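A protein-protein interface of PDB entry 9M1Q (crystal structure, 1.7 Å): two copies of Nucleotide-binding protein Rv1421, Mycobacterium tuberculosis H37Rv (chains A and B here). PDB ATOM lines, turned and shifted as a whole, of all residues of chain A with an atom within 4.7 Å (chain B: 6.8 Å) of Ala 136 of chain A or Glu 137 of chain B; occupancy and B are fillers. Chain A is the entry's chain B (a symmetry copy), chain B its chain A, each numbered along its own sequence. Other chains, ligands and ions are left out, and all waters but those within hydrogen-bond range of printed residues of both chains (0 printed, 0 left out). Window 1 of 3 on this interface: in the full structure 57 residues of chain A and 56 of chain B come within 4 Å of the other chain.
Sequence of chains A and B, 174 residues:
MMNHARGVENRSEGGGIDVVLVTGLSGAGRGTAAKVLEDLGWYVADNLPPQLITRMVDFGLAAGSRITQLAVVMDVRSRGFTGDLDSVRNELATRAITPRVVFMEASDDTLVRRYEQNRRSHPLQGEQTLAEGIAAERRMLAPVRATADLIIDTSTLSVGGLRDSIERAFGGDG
The backbone NH (N) of Gly 133 of chain B lies within hydrogen-bond range of the side-chain carboxylate (OE2) of Glu 137 of chain A, 3.4 Å away.
OE2 of Glu 137 of chain B sits at hydrogen-bond distance from OG of Ser 26 of chain A (2.8 Å).
The side-chain carboxylate of Glu 137 of chain B is in hydrogen-bond range of the backbone NH of Gly 133 of chain A.
Among the printed residues, merely in contact across the chains: Leu 25 of chain A with Glu 137 of chain B (3.6 Å), Leu 25 of chain A with Arg 138 of chain B (3.3 Å), Leu 25 of chain A with Leu 141 of chain B (3.9 Å), Glu 132 of chain A with Glu 137 of chain B (3.5 Å), Ala 136 of chain A with Ala 136 of chain B (3.8 Å), Ala 136 of chain A with Glu 137 of chain B (3.7 Å), Glu 137 of chain A with Glu 132 of chain B (3.5 Å), Glu 137 of chain A with Ala 136 of chain B (3.7 Å) and Met 140 of chain A with Ala 136 of chain B (3.97 Å).
Of the printed residues of chain B, Ser 26 of chain A touches Glu 137.
Ala 136 of chain A touches just these residues of chain B: Ala 136 (3.8 Å) and Glu 137 (3.7 Å).
Printed residues of chain B within 4 Å of Glu 137 of chain A: Glu 132 (3.5 Å), Gly 133 (3.4 Å) and Ala 136 (3.7 Å).
Of the printed residues of chain A, Arg 138 of chain B touches Leu 25.
Met 140 of chain B touches none of the printed residues of chain A.
Of the 11 printed residues of chain B, 6 touch a printed residue of chain A.
Hydrophobic or aromatic side chains of chain B within 4 Å of the printed part of chain A: Ala 136 and Leu 141.
Glu 132 of chain A touches Glu 137 of chain B, and with the chains exchanged Glu 137 of chain A touches Glu 132 of chain B.
Gly 133 of chain A touches Glu 137 of chain B, and with the chains exchanged Glu 137 of chain A touches Gly 133 of chain B.
Ala 136 of chain A touches its own counterpart, Ala 136 of chain B.
Ala 136 of chain A touches Glu 137 of chain B, and with the chains exchanged Glu 137 of chain A touches Ala 136 of chain B.
Of the 12 pairs that touch across the chains among the printed residues, 7 have their exchanged pair printed and touching as well.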
ATOM      1  N   LEU A  25     -13.897 -13.474  25.520  1.00  0.00           N
ATOM      2  CA  LEU A  25     -12.863 -12.453  25.639  1.00  0.00           C
ATOM      3  C   LEU A  25     -12.924 -11.760  27.000  1.00  0.00           C
ATOM      4  O   LEU A  25     -13.984 -11.660  27.625  1.00  0.00           O
ATOM      5  CB  LEU A  25     -13.016 -11.429  24.516  1.00  0.00           C
ATOM      6  CG  LEU A  25     -13.125 -12.062  23.124  1.00  0.00           C
ATOM      7  CD1 LEU A  25     -13.396 -10.987  22.064  1.00  0.00           C
ATOM      8  CD2 LEU A  25     -11.879 -12.885  22.771  1.00  0.00           C
ATOM      9  N   SER A  26     -11.758 -11.287  27.464  1.00  0.00           N
ATOM     10  CA  SER A  26     -11.693 -10.495  28.696  1.00  0.00           C
ATOM     11  C   SER A  26     -12.598  -9.272  28.604  1.00  0.00           C
ATOM     12  O   SER A  26     -12.466  -8.460  27.687  1.00  0.00           O
ATOM     13  CB  SER A  26     -10.246 -10.033  28.935  1.00  0.00           C
ATOM     14  OG  SER A  26      -9.359 -11.133  29.042  1.00  0.00           O
ATOM     15  N   THR A 129      -7.361  -8.776  33.510  1.00  0.00           N
ATOM     16  CA  THR A 129      -7.509  -8.577  32.067  1.00  0.00           C
ATOM     17  C   THR A 129      -6.150  -8.435  31.387  1.00  0.00           C
ATOM     18  O   THR A 129      -5.911  -9.015  30.316  1.00  0.00           O
ATOM     19  CB  THR A 129      -8.368  -7.340  31.797  1.00  0.00           C
ATOM     20  OG1 THR A 129      -9.720  -7.616  32.187  1.00  0.00           O
ATOM     21  CG2 THR A 129      -8.342  -6.956  30.320  1.00  0.00           C
ATOM     22  N   GLU A 132      -4.627 -11.899  31.292  1.00  0.00           N
ATOM     23  CA  GLU A 132      -5.202 -12.748  30.253  1.00  0.00           C
ATOM     24  C   GLU A 132      -4.658 -12.386  28.875  1.00  0.00           C
ATOM     25  O   GLU A 132      -4.393 -13.273  28.049  1.00  0.00           O
ATOM     26  CB  GLU A 132      -6.742 -12.647  30.278  1.00  0.00           C
ATOM     27  CG  GLU A 132      -7.352 -13.283  31.553  1.00  0.00           C
ATOM     28  CD  GLU A 132      -8.861 -13.073  31.725  1.00  0.00           C
ATOM     29  OE1 GLU A 132      -9.473 -13.815  32.536  1.00  0.00           O
ATOM     30  OE2 GLU A 132      -9.435 -12.172  31.077  1.00  0.00           O
ATOM     31  N   GLY A 133      -4.495 -11.092  28.602  1.00  0.00           N
ATOM     32  CA  GLY A 133      -3.937 -10.685  27.327  1.00  0.00           C
ATOM     33  C   GLY A 133      -2.502 -11.156  27.148  1.00  0.00           C
ATOM     34  O   GLY A 133      -2.125 -11.623  26.068  1.00  0.00           O
ATOM     35  N   ILE A 134      -1.684 -11.038  28.199  1.00  0.00           N
ATOM     36  CA  ILE A 134      -0.283 -11.468  28.086  1.00  0.00           C
ATOM     37  C   ILE A 134      -0.207 -12.987  27.950  1.00  0.00           C
ATOM     38  O   ILE A 134       0.593 -13.515  27.166  1.00  0.00           O
ATOM     39  CB  ILE A 134       0.552 -10.970  29.285  1.00  0.00           C
ATOM     40  CG1 ILE A 134       0.464  -9.446  29.405  1.00  0.00           C
ATOM     41  CG2 ILE A 134       2.024 -11.399  29.130  1.00  0.00           C
ATOM     42  CD1 ILE A 134       0.833  -8.878  30.794  1.00  0.00           C
ATOM     43  N   ALA A 135      -1.049 -13.713  28.692  1.00  0.00           N
ATOM     44  CA  ALA A 135      -1.062 -15.172  28.571  1.00  0.00           C
ATOM     45  C   ALA A 135      -1.434 -15.605  27.158  1.00  0.00           C
ATOM     46  O   ALA A 135      -0.839 -16.539  26.605  1.00  0.00           O
ATOM     47  CB  ALA A 135      -2.021 -15.782  29.597  1.00  0.00           C
ATOM     48  N   ALA A 136      -2.420 -14.938  26.553  1.00  0.00           N
ATOM     49  CA  ALA A 136      -2.774 -15.261  25.176  1.00  0.00           C
ATOM     50  C   ALA A 136      -1.622 -14.962  24.221  1.00  0.00           C
ATOM     51  O   ALA A 136      -1.372 -15.734  23.287  1.00  0.00           O
ATOM     52  CB  ALA A 136      -4.029 -14.496  24.743  1.00  0.00           C
ATOM     53  N   GLU A 137      -0.924 -13.835  24.415  1.00  0.00           N
ATOM     54  CA  GLU A 137       0.227 -13.548  23.559  1.00  0.00           C
ATOM     55  C   GLU A 137       1.284 -14.626  23.697  1.00  0.00           C
ATOM     56  O   GLU A 137       1.874 -15.055  22.697  1.00  0.00           O
ATOM     57  CB  GLU A 137       0.856 -12.188  23.891  1.00  0.00           C
ATOM     58  CG  GLU A 137      -0.010 -11.004  23.528  1.00  0.00           C
ATOM     59  CD  GLU A 137       0.719  -9.694  23.675  1.00  0.00           C
ATOM     60  OE1 GLU A 137       1.964  -9.708  23.893  1.00  0.00           O
ATOM     61  OE2 GLU A 137       0.039  -8.651  23.576  1.00  0.00           O
ATOM     62  N   ARG A 138       1.577 -15.037  24.935  1.00  0.00           N
ATOM     63  CA  ARG A 138       2.593 -16.072  25.130  1.00  0.00           C
ATOM     64  C   ARG A 138       2.186 -17.369  24.442  1.00  0.00           C
ATOM     65  O   ARG A 138       3.013 -18.028  23.801  1.00  0.00           O
ATOM     66  CB  ARG A 138       2.835 -16.333  26.615  1.00  0.00           C
ATOM     67  CG  ARG A 138       3.493 -15.189  27.380  1.00  0.00           C
ATOM     68  CD  ARG A 138       3.797 -15.617  28.801  1.00  0.00           C
ATOM     69  NE  ARG A 138       4.115 -14.489  29.662  1.00  0.00           N
ATOM     70  CZ  ARG A 138       5.317 -13.952  29.786  1.00  0.00           C
ATOM     71  NH1 ARG A 138       6.352 -14.410  29.100  1.00  0.00           N
ATOM     72  NH2 ARG A 138       5.483 -12.927  30.620  1.00  0.00           N
ATOM     73  N   ARG A 139       0.919 -17.775  24.594  1.00  0.00           N
ATOM     74  CA  ARG A 139       0.466 -18.995  23.925  1.00  0.00           C
ATOM     75  C   ARG A 139       0.523 -18.853  22.406  1.00  0.00           C
ATOM     76  O   ARG A 139       0.947 -19.780  21.705  1.00  0.00           O
ATOM     77  CB  ARG A 139      -0.950 -19.356  24.395  1.00  0.00           C
ATOM     78  CG  ARG A 139      -1.557 -20.541  23.642  1.00  0.00           C
ATOM     79  CD  ARG A 139      -1.173 -21.877  24.262  1.00  0.00           C
ATOM     80  NE  ARG A 139      -0.208 -22.622  23.460  1.00  0.00           N
ATOM     81  CZ  ARG A 139       0.984 -23.014  23.893  1.00  0.00           C
ATOM     82  NH1 ARG A 139       1.395 -22.743  25.123  1.00  0.00           N
ATOM     83  NH2 ARG A 139       1.776 -23.711  23.080  1.00  0.00           N
ATOM     84  N   MET A 140       0.112 -17.699  21.872  1.00  0.00           N
ATOM     85  CA  MET A 140       0.091 -17.530  20.428  1.00  0.00           C
ATOM     86  C   MET A 140       1.497 -17.507  19.848  1.00  0.00           C
ATOM     87  O   MET A 140       1.711 -17.998  18.740  1.00  0.00           O
ATOM     88  CB  MET A 140      -0.641 -16.238  20.054  1.00  0.00           C
ATOM     89  CG  MET A 140      -0.610 -15.889  18.590  1.00  0.00           C
ATOM     90  SD  MET A 140      -1.425 -14.317  18.221  1.00  0.00           S
ATOM     91  CE  MET A 140      -0.196 -13.136  18.765  1.00  0.00           C
ATOM     92  N   GLU B 132      -3.085  -5.486  20.936  1.00  0.00           N
ATOM     93  CA  GLU B 132      -2.334  -6.715  20.696  1.00  0.00           C
ATOM     94  C   GLU B 132      -2.796  -7.839  21.620  1.00  0.00           C
ATOM     95  O   GLU B 132      -2.911  -8.997  21.193  1.00  0.00           O
ATOM     96  CB  GLU B 132      -0.824  -6.443  20.860  1.00  0.00           C
ATOM     97  CG  GLU B 132      -0.265  -5.592  19.697  1.00  0.00           C
ATOM     98  CD  GLU B 132       1.167  -5.084  19.903  1.00  0.00           C
ATOM     99  OE1 GLU B 132       1.672  -5.130  21.042  1.00  0.00           O
ATOM    100  OE2 GLU B 132       1.784  -4.625  18.910  1.00  0.00           O
ATOM    101  N   GLY B 133      -3.067  -7.517  22.882  1.00  0.00           N
ATOM    102  CA  GLY B 133      -3.606  -8.514  23.792  1.00  0.00           C
ATOM    103  C   GLY B 133      -4.959  -9.047  23.351  1.00  0.00           C
ATOM    104  O   GLY B 133      -5.203 -10.255  23.412  1.00  0.00           O
ATOM    105  N   ILE B 134      -5.861  -8.156  22.922  1.00  0.00           N
ATOM    106  CA  ILE B 134      -7.187  -8.611  22.484  1.00  0.00           C
ATOM    107  C   ILE B 134      -7.074  -9.421  21.195  1.00  0.00           C
ATOM    108  O   ILE B 134      -7.768 -10.436  21.022  1.00  0.00           O
ATOM    109  CB  ILE B 134      -8.157  -7.425  22.312  1.00  0.00           C
ATOM    110  CG1 ILE B 134      -8.268  -6.629  23.618  1.00  0.00           C
ATOM    111  CG2 ILE B 134      -9.535  -7.949  21.839  1.00  0.00           C
ATOM    112  CD1 ILE B 134      -8.850  -5.190  23.465  1.00  0.00           C
ATOM    113  N   ALA B 135      -6.202  -8.996  20.273  1.00  0.00           N
ATOM    114  CA  ALA B 135      -6.015  -9.765  19.045  1.00  0.00           C
ATOM    115  C   ALA B 135      -5.485 -11.157  19.352  1.00  0.00           C
ATOM    116  O   ALA B 135      -5.921 -12.143  18.749  1.00  0.00           O
ATOM    117  CB  ALA B 135      -5.086  -9.022  18.083  1.00  0.00           C
ATOM    118  N   ALA B 136      -4.567 -11.271  20.315  1.00  0.00           N
ATOM    119  CA  ALA B 136      -4.078 -12.602  20.671  1.00  0.00           C
ATOM    120  C   ALA B 136      -5.184 -13.460  21.286  1.00  0.00           C
ATOM    121  O   ALA B 136      -5.268 -14.663  21.004  1.00  0.00           O
ATOM    122  CB  ALA B 136      -2.881 -12.506  21.620  1.00  0.00           C
ATOM    123  N   GLU B 137      -6.034 -12.866  22.136  1.00  0.00           N
ATOM    124  CA  GLU B 137      -7.157 -13.622  22.696  1.00  0.00           C
ATOM    125  C   GLU B 137      -8.080 -14.122  21.595  1.00  0.00           C
ATOM    126  O   GLU B 137      -8.543 -15.270  21.640  1.00  0.00           O
ATOM    127  CB  GLU B 137      -7.963 -12.779  23.695  1.00  0.00           C
ATOM    128  CG  GLU B 137      -7.204 -12.484  24.975  1.00  0.00           C
ATOM    129  CD  GLU B 137      -8.054 -11.832  26.034  1.00  0.00           C
ATOM    130  OE1 GLU B 137      -9.304 -11.821  25.897  1.00  0.00           O
ATOM    131  OE2 GLU B 137      -7.462 -11.316  27.003  1.00  0.00           O
ATOM    132  N   ARG B 138      -8.412 -13.255  20.633  1.00  0.00           N
ATOM    133  CA  ARG B 138      -9.311 -13.667  19.552  1.00  0.00           C
ATOM    134  C   ARG B 138      -8.716 -14.815  18.745  1.00  0.00           C
ATOM    135  O   ARG B 138      -9.421 -15.767  18.383  1.00  0.00           O
ATOM    136  CB  ARG B 138      -9.614 -12.490  18.629  1.00  0.00           C
ATOM    137  CG  ARG B 138     -10.462 -11.378  19.257  1.00  0.00           C
ATOM    138  CD  ARG B 138     -10.874 -10.384  18.183  1.00  0.00           C
ATOM    139  NE  ARG B 138     -11.356  -9.131  18.742  1.00  0.00           N
ATOM    140  CZ  ARG B 138     -12.612  -8.916  19.088  1.00  0.00           C
ATOM    141  NH1 ARG B 138     -13.535  -9.852  18.930  1.00  0.00           N
ATOM    142  NH2 ARG B 138     -12.949  -7.733  19.603  1.00  0.00           N
ATOM    143  N   ARG B 139      -7.424 -14.729  18.419  1.00  0.00           N
ATOM    144  CA  ARG B 139      -6.794 -15.823  17.681  1.00  0.00           C
ATOM    145  C   ARG B 139      -6.751 -17.107  18.508  1.00  0.00           C
ATOM    146  O   ARG B 139      -7.043 -18.199  17.994  1.00  0.00           O
ATOM    147  CB  ARG B 139      -5.384 -15.395  17.237  1.00  0.00           C
ATOM    148  CG  ARG B 139      -4.624 -16.468  16.455  1.00  0.00           C
ATOM    149  CD  ARG B 139      -5.051 -16.532  14.989  1.00  0.00           C
ATOM    150  NE  ARG B 139      -5.869 -17.702  14.681  1.00  0.00           N
ATOM    151  CZ  ARG B 139      -7.103 -17.648  14.195  1.00  0.00           C
ATOM    152  NH1 ARG B 139      -7.705 -16.491  13.965  1.00  0.00           N
ATOM    153  NH2 ARG B 139      -7.741 -18.784  13.914  1.00  0.00           N
ATOM    154  N   MET B 140      -6.401 -17.007  19.794  1.00  0.00           N
ATOM    155  CA  MET B 140      -6.311 -18.195  20.637  1.00  0.00           C
ATOM    156  C   MET B 140      -7.667 -18.848  20.840  1.00  0.00           C
ATOM    157  O   MET B 140      -7.747 -20.075  20.952  1.00  0.00           O
ATOM    158  CB  MET B 140      -5.708 -17.850  22.005  1.00  0.00           C
ATOM    159  CG  MET B 140      -5.652 -19.002  22.989  1.00  0.00           C
ATOM    160  SD  MET B 140      -5.162 -18.506  24.663  1.00  0.00           S
ATOM    161  CE  MET B 140      -6.632 -17.658  25.236  1.00  0.00           C
ATOM    162  N   LEU B 141      -8.730 -18.051  20.913  1.00  0.00           N
ATOM    163  CA  LEU B 141     -10.057 -18.593  21.171  1.00  0.00           C
ATOM    164  C   LEU B 141     -10.820 -18.943  19.897  1.00  0.00           C
ATOM    165  O   LEU B 141     -11.956 -19.438  19.990  1.00  0.00           O
ATOM    166  CB  LEU B 141     -10.859 -17.610  22.016  1.00  0.00           C
ATOM    167  CG  LEU B 141     -10.413 -17.605  23.486  1.00  0.00           C
ATOM    168  CD1 LEU B 141     -11.102 -16.481  24.193  1.00  0.00           C
ATOM    169  CD2 LEU B 141     -10.737 -18.921  24.145  1.00  0.00           C
ATOM    170  N   ALA B 142     -10.222 -18.735  18.723  1.00  0.00           N
ATOM    171  CA  ALA B 142     -10.956 -18.977  17.482  1.00  0.00           C
ATOM    172  C   ALA B 142     -11.469 -20.409  17.353  1.00  0.00           C
ATOM    173  O   ALA B 142     -12.627 -20.579  16.929  1.00  0.00           O
ATOM    174  CB  ALA B 142     -10.089 -18.586  16.269  1.00  0.00           C
